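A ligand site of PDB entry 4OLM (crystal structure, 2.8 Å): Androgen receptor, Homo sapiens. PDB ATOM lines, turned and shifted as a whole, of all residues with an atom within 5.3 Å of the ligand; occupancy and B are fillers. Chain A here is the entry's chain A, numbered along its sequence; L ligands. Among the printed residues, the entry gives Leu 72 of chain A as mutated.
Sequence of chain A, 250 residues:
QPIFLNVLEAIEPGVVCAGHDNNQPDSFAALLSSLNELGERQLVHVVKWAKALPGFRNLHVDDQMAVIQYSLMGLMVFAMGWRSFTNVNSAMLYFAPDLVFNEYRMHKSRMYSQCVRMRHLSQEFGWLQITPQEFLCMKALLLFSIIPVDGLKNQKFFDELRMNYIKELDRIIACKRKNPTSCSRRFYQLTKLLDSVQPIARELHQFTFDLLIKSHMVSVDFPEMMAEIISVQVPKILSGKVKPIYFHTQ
An oxygen (O3) of the ligand lies close to the backbone NH (N) of Asn 36 (3.0 Å).
OD1 of Asn 36 sits at hydrogen-bond distance from O3 of the ligand.
O of Leu 35 lies within hydrogen-bond range of O3 of the ligand, 2.6 Å away.
NH2 of Arg 83 lies within hydrogen-bond range of N2 of the ligand (2.6 Å).
The side-chain amide nitrogen (NE2) of Gln 42 lies within hydrogen-bond range of a nitrogen (N2) of the ligand, 3.3 Å away.
The side-chain amide oxygen (OD1) of Asn 36 lies close to the backbone carbonyl oxygen (O) of Leu 32 (3.1 Å).
NH2 of Arg 83 is in hydrogen-bond range of OE1 of Gln 42, 3.2 Å away.
NE of Arg 83 is in hydrogen-bond range of O of Phe 95, 3.3 Å away.
NE2 of Gln 42 sits close to SD of Met 76 (3.8 Å).
The backbone carbonyl oxygen (O) of Phe 95 sits close to the side-chain amide oxygen (OE1) of Gln 42, at 3.2 Å.
OG1 of Thr 208 lies within hydrogen-bond range of O of Leu 204, at 2.6 Å.
SD of Met 80 sits close to N of Phe 95 (3.7 Å).
The backbone NH (N) of Val 234 sits at hydrogen-bond distance from the backbone carbonyl oxygen (O) of Ile 229, at 2.7 Å.
The side-chain sulfur of Met 73 sits close to an oxygen (O4) of the ligand, at 3.3 Å.
The backbone NH of Val 77 lies close to a fluorine (F2) of the ligand (2.9 Å).
F4 of the ligand lies close to SD of Met 118 (3.6 Å).
A ring nitrogen (NE2) of His 205 sits close to a fluorine (F1) of the ligand (3.4 Å).
Leu 38 touches the ligand (CD2 to C14, 3.5 Å).
Gly 39 touches the ligand.
CD2 of Leu 72 touches C3 of the ligand, 3.6 Å away.
CB of Met 76 touches F2 of the ligand, 3.3 Å away.
Met 80 touches the ligand.
CD2 of Phe 95 touches C16 of the ligand, at 3.5 Å.
Thr 208 touches the ligand.
Phe 222 touches the ligand.
CE of Met 226 touches C5 of the ligand, at 3.3 Å.
Ile 229 touches the ligand (CG2 to C4, 3.97 Å).
CG1 of Ile 230 touches C5 of the ligand, at 3.6 Å.
Val 234 touches the ligand (CG2 to F1, 3.7 Å).
20 residues have an atom within 4 Å of the ligand: Leu 35, Asn 36, Leu 38, Gly 39, Gln 42, Leu 72, Met 73, Met 76, Val 77, Met 80, Arg 83, Phe 95, Met 118, His 205, Thr 208, Phe 222, Met 226, Ile 229, Ile 230 and Val 234.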
ATOM      1  N   LEU A  32      -1.211 -10.706 -11.270  1.00  0.00           N
ATOM      2  CA  LEU A  32      -0.478  -9.443 -11.200  1.00  0.00           C
ATOM      3  C   LEU A  32       0.400  -9.093 -12.385  1.00  0.00           C
ATOM      4  O   LEU A  32       1.007  -8.020 -12.399  1.00  0.00           O
ATOM      5  CB  LEU A  32       0.299  -9.350  -9.888  1.00  0.00           C
ATOM      6  CG  LEU A  32      -0.753  -8.960  -8.834  1.00  0.00           C
ATOM      7  CD1 LEU A  32      -0.546  -9.730  -7.557  1.00  0.00           C
ATOM      8  CD2 LEU A  32      -0.760  -7.460  -8.588  1.00  0.00           C
ATOM      9  N   LEU A  35      -2.592  -7.102 -14.152  1.00  0.00           N
ATOM     10  CA  LEU A  35      -2.952  -5.781 -13.647  1.00  0.00           C
ATOM     11  C   LEU A  35      -1.892  -4.730 -13.956  1.00  0.00           C
ATOM     12  O   LEU A  35      -2.217  -3.530 -13.960  1.00  0.00           O
ATOM     13  CB  LEU A  35      -3.294  -5.817 -12.154  1.00  0.00           C
ATOM     14  CG  LEU A  35      -4.698  -6.381 -11.853  1.00  0.00           C
ATOM     15  CD1 LEU A  35      -4.757  -6.980 -10.463  1.00  0.00           C
ATOM     16  CD2 LEU A  35      -5.782  -5.331 -12.044  1.00  0.00           C
ATOM     17  N   ASN A  36      -0.653  -5.142 -14.227  1.00  0.00           N
ATOM     18  CA  ASN A  36       0.403  -4.178 -14.638  1.00  0.00           C
ATOM     19  C   ASN A  36       0.266  -3.858 -16.086  1.00  0.00           C
ATOM     20  O   ASN A  36       0.645  -2.781 -16.521  1.00  0.00           O
ATOM     21  CB  ASN A  36       1.813  -4.698 -14.366  1.00  0.00           C
ATOM     22  CG  ASN A  36       2.018  -5.131 -12.938  1.00  0.00           C
ATOM     23  OD1 ASN A  36       1.144  -4.943 -12.081  1.00  0.00           O
ATOM     24  ND2 ASN A  36       3.156  -5.739 -12.669  1.00  0.00           N
ATOM     25  N   GLU A  37      -0.306  -4.790 -16.849  1.00  0.00           N
ATOM     26  CA  GLU A  37      -0.500  -4.566 -18.270  1.00  0.00           C
ATOM     27  C   GLU A  37      -1.711  -3.703 -18.496  1.00  0.00           C
ATOM     28  O   GLU A  37      -1.664  -2.819 -19.366  1.00  0.00           O
ATOM     29  CB  GLU A  37      -0.651  -5.877 -19.050  1.00  0.00           C
ATOM     30  CG  GLU A  37      -0.386  -5.703 -20.547  1.00  0.00           C
ATOM     31  CD  GLU A  37       0.994  -5.130 -20.831  1.00  0.00           C
ATOM     32  OE1 GLU A  37       1.104  -4.216 -21.686  1.00  0.00           O
ATOM     33  OE2 GLU A  37       1.959  -5.575 -20.160  1.00  0.00           O
ATOM     34  N   LEU A  38      -2.769  -3.971 -17.708  1.00  0.00           N
ATOM     35  CA  LEU A  38      -4.009  -3.166 -17.674  1.00  0.00           C
ATOM     36  C   LEU A  38      -3.752  -1.753 -17.181  1.00  0.00           C
ATOM     37  O   LEU A  38      -4.318  -0.783 -17.724  1.00  0.00           O
ATOM     38  CB  LEU A  38      -5.070  -3.828 -16.781  1.00  0.00           C
ATOM     39  CG  LEU A  38      -6.460  -3.166 -16.622  1.00  0.00           C
ATOM     40  CD1 LEU A  38      -7.217  -2.967 -17.943  1.00  0.00           C
ATOM     41  CD2 LEU A  38      -7.292  -4.012 -15.652  1.00  0.00           C
ATOM     42  N   GLY A  39      -2.922  -1.633 -16.150  1.00  0.00           N
ATOM     43  CA  GLY A  39      -2.512  -0.321 -15.657  1.00  0.00           C
ATOM     44  C   GLY A  39      -1.869   0.530 -16.747  1.00  0.00           C
ATOM     45  O   GLY A  39      -2.158   1.735 -16.846  1.00  0.00           O
ATOM     46  N   GLU A  40      -1.007  -0.102 -17.552  1.00  0.00           N
ATOM     47  CA  GLU A  40      -0.317   0.559 -18.668  1.00  0.00           C
ATOM     48  C   GLU A  40      -1.281   0.854 -19.772  1.00  0.00           C
ATOM     49  O   GLU A  40      -1.220   1.944 -20.363  1.00  0.00           O
ATOM     50  CB  GLU A  40       0.807  -0.309 -19.234  1.00  0.00           C
ATOM     51  CG  GLU A  40       1.820   0.524 -20.022  1.00  0.00           C
ATOM     52  CD  GLU A  40       2.517  -0.235 -21.124  1.00  0.00           C
ATOM     53  OE1 GLU A  40       3.672   0.115 -21.398  1.00  0.00           O
ATOM     54  OE2 GLU A  40       1.898  -1.155 -21.709  1.00  0.00           O
ATOM     55  N   GLN A  42      -4.679   1.188 -19.271  1.00  0.00           N
ATOM     56  CA  GLN A  42      -5.527   2.270 -18.749  1.00  0.00           C
ATOM     57  C   GLN A  42      -4.742   3.585 -18.761  1.00  0.00           C
ATOM     58  O   GLN A  42      -5.249   4.597 -19.248  1.00  0.00           O
ATOM     59  CB  GLN A  42      -6.154   1.934 -17.371  1.00  0.00           C
ATOM     60  CG  GLN A  42      -7.286   0.891 -17.485  1.00  0.00           C
ATOM     61  CD  GLN A  42      -8.160   0.680 -16.247  1.00  0.00           C
ATOM     62  OE1 GLN A  42      -8.943  -0.293 -16.207  1.00  0.00           O
ATOM     63  NE2 GLN A  42      -8.009   1.535 -15.232  1.00  0.00           N
ATOM     64  N   GLN A  69       1.164  11.123 -13.504  1.00  0.00           N
ATOM     65  CA  GLN A  69       1.852   9.991 -12.883  1.00  0.00           C
ATOM     66  C   GLN A  69       1.464   9.939 -11.425  1.00  0.00           C
ATOM     67  O   GLN A  69       1.273   8.867 -10.844  1.00  0.00           O
ATOM     68  CB  GLN A  69       3.363  10.086 -13.081  1.00  0.00           C
ATOM     69  CG  GLN A  69       3.726  10.061 -14.565  1.00  0.00           C
ATOM     70  CD  GLN A  69       5.154  10.487 -14.828  1.00  0.00           C
ATOM     71  OE1 GLN A  69       5.467  11.693 -14.926  1.00  0.00           O
ATOM     72  NE2 GLN A  69       6.036   9.507 -14.987  1.00  0.00           N
ATOM     73  N   LEU A  72      -2.478   8.856 -11.258  1.00  0.00           N
ATOM     74  CA  LEU A  72      -2.865   7.730 -12.159  1.00  0.00           C
ATOM     75  C   LEU A  72      -3.557   6.621 -11.422  1.00  0.00           C
ATOM     76  O   LEU A  72      -4.628   6.203 -11.797  1.00  0.00           O
ATOM     77  CB  LEU A  72      -1.643   7.142 -12.907  1.00  0.00           C
ATOM     78  CG  LEU A  72      -1.753   5.661 -13.376  1.00  0.00           C
ATOM     79  CD1 LEU A  72      -2.629   5.543 -14.595  1.00  0.00           C
ATOM     80  CD2 LEU A  72      -0.411   5.025 -13.667  1.00  0.00           C
ATOM     81  N   MET A  73      -2.929   6.122 -10.377  1.00  0.00           N
ATOM     82  CA  MET A  73      -3.534   5.023  -9.597  1.00  0.00           C
ATOM     83  C   MET A  73      -4.940   5.388  -9.084  1.00  0.00           C
ATOM     84  O   MET A  73      -5.879   4.642  -9.365  1.00  0.00           O
ATOM     85  CB  MET A  73      -2.635   4.626  -8.401  1.00  0.00           C
ATOM     86  CG  MET A  73      -3.057   3.348  -7.682  1.00  0.00           C
ATOM     87  SD  MET A  73      -2.934   1.819  -8.626  1.00  0.00           S
ATOM     88  CE  MET A  73      -1.428   1.175  -7.888  1.00  0.00           C
ATOM     89  N   MET A  76      -7.725   5.288 -11.529  1.00  0.00           N
ATOM     90  CA  MET A  76      -8.038   3.969 -12.098  1.00  0.00           C
ATOM     91  C   MET A  76      -9.022   3.223 -11.213  1.00  0.00           C
ATOM     92  O   MET A  76     -10.056   2.734 -11.676  1.00  0.00           O
ATOM     93  CB  MET A  76      -6.762   3.147 -12.269  1.00  0.00           C
ATOM     94  CG  MET A  76      -5.722   3.784 -13.178  1.00  0.00           C
ATOM     95  SD  MET A  76      -4.623   2.578 -13.914  1.00  0.00           S
ATOM     96  CE  MET A  76      -4.160   1.616 -12.482  1.00  0.00           C
ATOM     97  N   VAL A  77      -8.645   3.106  -9.957  1.00  0.00           N
ATOM     98  CA  VAL A  77      -9.563   2.801  -8.869  1.00  0.00           C
ATOM     99  C   VAL A  77     -10.950   3.445  -8.983  1.00  0.00           C
ATOM    100  O   VAL A  77     -11.975   2.774  -8.816  1.00  0.00           O
ATOM    101  CB  VAL A  77      -8.986   3.358  -7.554  1.00  0.00           C
ATOM    102  CG1 VAL A  77     -10.073   3.505  -6.485  1.00  0.00           C
ATOM    103  CG2 VAL A  77      -7.834   2.482  -7.064  1.00  0.00           C
ATOM    104  N   MET A  80     -12.868   2.109 -11.732  1.00  0.00           N
ATOM    105  CA  MET A  80     -13.175   0.757 -11.332  1.00  0.00           C
ATOM    106  C   MET A  80     -14.281   0.835 -10.267  1.00  0.00           C
ATOM    107  O   MET A  80     -15.201   0.013 -10.249  1.00  0.00           O
ATOM    108  CB  MET A  80     -11.915   0.119 -10.773  1.00  0.00           C
ATOM    109  CG  MET A  80     -11.852  -1.340 -11.107  1.00  0.00           C
ATOM    110  SD  MET A  80     -12.525  -2.337  -9.801  1.00  0.00           S
ATOM    111  CE  MET A  80     -11.252  -2.116  -8.560  1.00  0.00           C
ATOM    112  N   ARG A  83     -16.930   1.118 -12.845  1.00  0.00           N
ATOM    113  CA  ARG A  83     -17.104  -0.098 -13.638  1.00  0.00           C
ATOM    114  C   ARG A  83     -17.661  -1.268 -12.771  1.00  0.00           C
ATOM    115  O   ARG A  83     -18.628  -1.941 -13.149  1.00  0.00           O
ATOM    116  CB  ARG A  83     -15.772  -0.492 -14.291  1.00  0.00           C
ATOM    117  CG  ARG A  83     -15.306   0.242 -15.573  1.00  0.00           C
ATOM    118  CD  ARG A  83     -13.996  -0.410 -16.185  1.00  0.00           C
ATOM    119  NE  ARG A  83     -12.925  -0.503 -15.188  1.00  0.00           N
ATOM    120  CZ  ARG A  83     -12.074   0.458 -15.021  1.00  0.00           C
ATOM    121  NH1 ARG A  83     -12.168   1.475 -15.783  1.00  0.00           N
ATOM    122  NH2 ARG A  83     -11.166   0.427 -14.086  1.00  0.00           N
ATOM    123  N   PHE A  95     -12.279  -4.392 -12.902  1.00  0.00           N
ATOM    124  CA  PHE A  95     -11.038  -3.835 -13.439  1.00  0.00           C
ATOM    125  C   PHE A  95     -11.138  -3.864 -14.965  1.00  0.00           C
ATOM    126  O   PHE A  95     -10.690  -2.939 -15.685  1.00  0.00           O
ATOM    127  CB  PHE A  95      -9.895  -4.776 -13.103  1.00  0.00           C
ATOM    128  CG  PHE A  95      -9.557  -4.884 -11.639  1.00  0.00           C
ATOM    129  CD1 PHE A  95      -9.936  -6.008 -10.912  1.00  0.00           C
ATOM    130  CD2 PHE A  95      -8.772  -3.952 -11.049  1.00  0.00           C
ATOM    131  CE1 PHE A  95      -9.557  -6.135  -9.576  1.00  0.00           C
ATOM    132  CE2 PHE A  95      -8.373  -4.098  -9.729  1.00  0.00           C
ATOM    133  CZ  PHE A  95      -8.770  -5.183  -8.994  1.00  0.00           C
ATOM    134  N   MET A 111      -3.764  -8.984  -2.483  1.00  0.00           N
ATOM    135  CA  MET A 111      -4.132  -7.574  -2.448  1.00  0.00           C
ATOM    136  C   MET A 111      -5.452  -7.420  -1.700  1.00  0.00           C
ATOM    137  O   MET A 111      -6.159  -6.431  -1.930  1.00  0.00           O
ATOM    138  CB  MET A 111      -4.311  -7.034  -3.880  1.00  0.00           C
ATOM    139  CG  MET A 111      -3.157  -6.196  -4.407  1.00  0.00           C
ATOM    140  SD  MET A 111      -3.326  -5.687  -6.130  1.00  0.00           S
ATOM    141  CE  MET A 111      -4.036  -4.055  -5.971  1.00  0.00           C
ATOM    142  N   MET A 118     -11.686  -1.142  -2.075  1.00  0.00           N
ATOM    143  CA  MET A 118     -12.190  -0.774  -3.410  1.00  0.00           C
ATOM    144  C   MET A 118     -13.633  -1.218  -3.709  1.00  0.00           C
ATOM    145  O   MET A 118     -14.290  -0.585  -4.547  1.00  0.00           O
ATOM    146  CB  MET A 118     -11.292  -1.331  -4.511  1.00  0.00           C
ATOM    147  CG  MET A 118      -9.928  -0.661  -4.605  1.00  0.00           C
ATOM    148  SD  MET A 118      -9.084  -0.993  -6.153  1.00  0.00           S
ATOM    149  CE  MET A 118      -8.467  -2.652  -5.835  1.00  0.00           C
ATOM    150  N   LEU A 204      -2.060   0.767  -2.314  1.00  0.00           N
ATOM    151  CA  LEU A 204      -1.802   0.037  -3.515  1.00  0.00           C
ATOM    152  C   LEU A 204      -0.396   0.448  -3.889  1.00  0.00           C
ATOM    153  O   LEU A 204       0.473  -0.398  -4.069  1.00  0.00           O
ATOM    154  CB  LEU A 204      -2.801   0.433  -4.599  1.00  0.00           C
ATOM    155  CG  LEU A 204      -4.314   0.210  -4.368  1.00  0.00           C
ATOM    156  CD1 LEU A 204      -5.115   1.156  -5.237  1.00  0.00           C
ATOM    157  CD2 LEU A 204      -4.767  -1.208  -4.665  1.00  0.00           C
ATOM    158  N   HIS A 205      -0.177   1.756  -3.975  1.00  0.00           N
ATOM    159  CA  HIS A 205       1.153   2.274  -4.264  1.00  0.00           C
ATOM    160  C   HIS A 205       2.220   1.600  -3.395  1.00  0.00           C
ATOM    161  O   HIS A 205       3.358   1.416  -3.841  1.00  0.00           O
ATOM    162  CB  HIS A 205       1.182   3.791  -4.048  1.00  0.00           C
ATOM    163  CG  HIS A 205       0.587   4.576  -5.170  1.00  0.00           C
ATOM    164  ND1 HIS A 205      -0.341   5.574  -4.978  1.00  0.00           N
ATOM    165  CD2 HIS A 205       0.789   4.509  -6.512  1.00  0.00           C
ATOM    166  CE1 HIS A 205      -0.694   6.081  -6.149  1.00  0.00           C
ATOM    167  NE2 HIS A 205      -0.024   5.455  -7.095  1.00  0.00           N
ATOM    168  N   THR A 208       2.514  -2.088  -4.780  1.00  0.00           N
ATOM    169  CA  THR A 208       3.122  -2.000  -6.082  1.00  0.00           C
ATOM    170  C   THR A 208       4.610  -1.812  -5.917  1.00  0.00           C
ATOM    171  O   THR A 208       5.394  -2.601  -6.405  1.00  0.00           O
ATOM    172  CB  THR A 208       2.594  -0.760  -6.829  1.00  0.00           C
ATOM    173  OG1 THR A 208       1.205  -0.589  -6.541  1.00  0.00           O
ATOM    174  CG2 THR A 208       2.836  -0.921  -8.315  1.00  0.00           C
ATOM    175  N   LEU A 211       6.113  -4.652  -4.609  1.00  0.00           N
ATOM    176  CA  LEU A 211       6.005  -5.727  -5.568  1.00  0.00           C
ATOM    177  C   LEU A 211       7.058  -5.571  -6.656  1.00  0.00           C
ATOM    178  O   LEU A 211       7.637  -6.535  -7.076  1.00  0.00           O
ATOM    179  CB  LEU A 211       4.596  -5.793  -6.155  1.00  0.00           C
ATOM    180  CG  LEU A 211       4.395  -6.793  -7.281  1.00  0.00           C
ATOM    181  CD1 LEU A 211       4.840  -8.202  -6.892  1.00  0.00           C
ATOM    182  CD2 LEU A 211       2.928  -6.769  -7.677  1.00  0.00           C
ATOM    183  N   PHE A 222       6.525  -6.687 -15.165  1.00  0.00           N
ATOM    184  CA  PHE A 222       6.304  -5.250 -15.194  1.00  0.00           C
ATOM    185  C   PHE A 222       6.613  -4.639 -16.535  1.00  0.00           C
ATOM    186  O   PHE A 222       7.679  -4.905 -17.086  1.00  0.00           O
ATOM    187  CB  PHE A 222       7.136  -4.529 -14.138  1.00  0.00           C
ATOM    188  CG  PHE A 222       6.342  -4.182 -12.921  1.00  0.00           C
ATOM    189  CD1 PHE A 222       6.647  -4.744 -11.696  1.00  0.00           C
ATOM    190  CD2 PHE A 222       5.246  -3.340 -13.032  1.00  0.00           C
ATOM    191  CE1 PHE A 222       5.891  -4.435 -10.585  1.00  0.00           C
ATOM    192  CE2 PHE A 222       4.476  -3.037 -11.937  1.00  0.00           C
ATOM    193  CZ  PHE A 222       4.799  -3.584 -10.695  1.00  0.00           C
ATOM    194  N   MET A 226       6.062   0.981 -16.641  1.00  0.00           N
ATOM    195  CA  MET A 226       5.447   1.112 -15.310  1.00  0.00           C
ATOM    196  C   MET A 226       6.472   1.104 -14.192  1.00  0.00           C
ATOM    197  O   MET A 226       6.303   1.783 -13.179  1.00  0.00           O
ATOM    198  CB  MET A 226       4.394   0.013 -15.089  1.00  0.00           C
ATOM    199  CG  MET A 226       3.225   0.091 -16.050  1.00  0.00           C
ATOM    200  SD  MET A 226       2.797   1.815 -16.414  1.00  0.00           S
ATOM    201  CE  MET A 226       2.309   2.397 -14.785  1.00  0.00           C
ATOM    202  N   ILE A 229       7.755   4.700 -13.452  1.00  0.00           N
ATOM    203  CA  ILE A 229       6.825   5.456 -12.612  1.00  0.00           C
ATOM    204  C   ILE A 229       6.850   4.965 -11.167  1.00  0.00           C
ATOM    205  O   ILE A 229       6.911   5.747 -10.218  1.00  0.00           O
ATOM    206  CB  ILE A 229       5.401   5.311 -13.158  1.00  0.00           C
ATOM    207  CG1 ILE A 229       5.285   5.935 -14.551  1.00  0.00           C
ATOM    208  CG2 ILE A 229       4.399   5.979 -12.207  1.00  0.00           C
ATOM    209  CD1 ILE A 229       4.192   5.332 -15.389  1.00  0.00           C
ATOM    210  N   ILE A 230       6.826   3.658 -11.011  1.00  0.00           N
ATOM    211  CA  ILE A 230       6.920   3.051  -9.710  1.00  0.00           C
ATOM    212  C   ILE A 230       8.230   3.363  -9.003  1.00  0.00           C
ATOM    213  O   ILE A 230       8.262   3.454  -7.782  1.00  0.00           O
ATOM    214  CB  ILE A 230       6.711   1.542  -9.783  1.00  0.00           C
ATOM    215  CG1 ILE A 230       5.329   1.239 -10.380  1.00  0.00           C
ATOM    216  CG2 ILE A 230       6.809   0.903  -8.406  1.00  0.00           C
ATOM    217  CD1 ILE A 230       5.241  -0.136 -10.985  1.00  0.00           C
ATOM    218  N   VAL A 234       6.317   7.261  -8.093  1.00  0.00           N
ATOM    219  CA  VAL A 234       5.572   6.664  -6.964  1.00  0.00           C
ATOM    220  C   VAL A 234       6.289   7.006  -5.641  1.00  0.00           C
ATOM    221  O   VAL A 234       5.662   7.539  -4.744  1.00  0.00           O
ATOM    222  CB  VAL A 234       5.282   5.120  -7.163  1.00  0.00           C
ATOM    223  CG1 VAL A 234       5.112   4.390  -5.853  1.00  0.00           C
ATOM    224  CG2 VAL A 234       4.036   4.876  -8.016  1.00  0.00           C
HETATM  225  C1  LIG L   1      -0.416   1.674 -11.072  1.00  0.00           C
HETATM  226  C2  LIG L   1      -0.302   2.981 -10.644  1.00  0.00           C
HETATM  227  C3  LIG L   1       0.917   3.623 -10.688  1.00  0.00           C
HETATM  228  F1  LIG L   1       1.048   4.891 -10.268  1.00  0.00           F
HETATM  229  C4  LIG L   1       2.034   2.963 -11.167  1.00  0.00           C
HETATM  230  C5  LIG L   1       1.928   1.653 -11.601  1.00  0.00           C
HETATM  231  C6  LIG L   1       0.696   1.016 -11.559  1.00  0.00           C
HETATM  232  S1  LIG L   1       0.562  -0.478 -12.053  1.00  0.00           S
HETATM  233  O1  LIG L   1      -0.621  -0.701 -12.832  1.00  0.00           O
HETATM  234  O2  LIG L   1       1.741  -0.803 -12.810  1.00  0.00           O
HETATM  235  C7  LIG L   1       0.452  -1.401 -10.679  1.00  0.00           C
HETATM  236  C8  LIG L   1      -0.642  -2.459 -10.785  1.00  0.00           C
HETATM  237  O3  LIG L   1      -0.490  -3.053 -12.082  1.00  0.00           O
HETATM  238  C9  LIG L   1      -0.476  -3.518  -9.705  1.00  0.00           C
HETATM  239  C10 LIG L   1      -2.063  -1.905 -10.680  1.00  0.00           C
HETATM  240  O4  LIG L   1      -2.438  -1.233  -9.731  1.00  0.00           O
HETATM  241  N1  LIG L   1      -2.854  -2.286 -11.674  1.00  0.00           N
HETATM  242  C11 LIG L   1      -4.140  -1.971 -11.806  1.00  0.00           C
HETATM  243  C12 LIG L   1      -4.868  -1.396 -10.785  1.00  0.00           C
HETATM  244  C13 LIG L   1      -4.710  -2.165 -13.044  1.00  0.00           C
HETATM  245  C14 LIG L   1      -6.012  -1.804 -13.312  1.00  0.00           C
HETATM  246  C15 LIG L   1      -6.793  -1.242 -12.322  1.00  0.00           C
HETATM  247  C16 LIG L   1      -7.983  -0.883 -12.614  1.00  0.00           C
HETATM  248  N2  LIG L   1      -9.044  -0.542 -12.897  1.00  0.00           N
HETATM  249  C17 LIG L   1      -6.185  -1.018 -10.993  1.00  0.00           C
HETATM  250  C18 LIG L   1      -6.956  -0.403  -9.875  1.00  0.00           C
HETATM  251  F2  LIG L   1      -6.706   0.896  -9.826  1.00  0.00           F
HETATM  252  F3  LIG L   1      -8.234  -0.578 -10.135  1.00  0.00           F
HETATM  253  F4  LIG L   1      -6.593  -1.022  -8.736  1.00  0.00           F
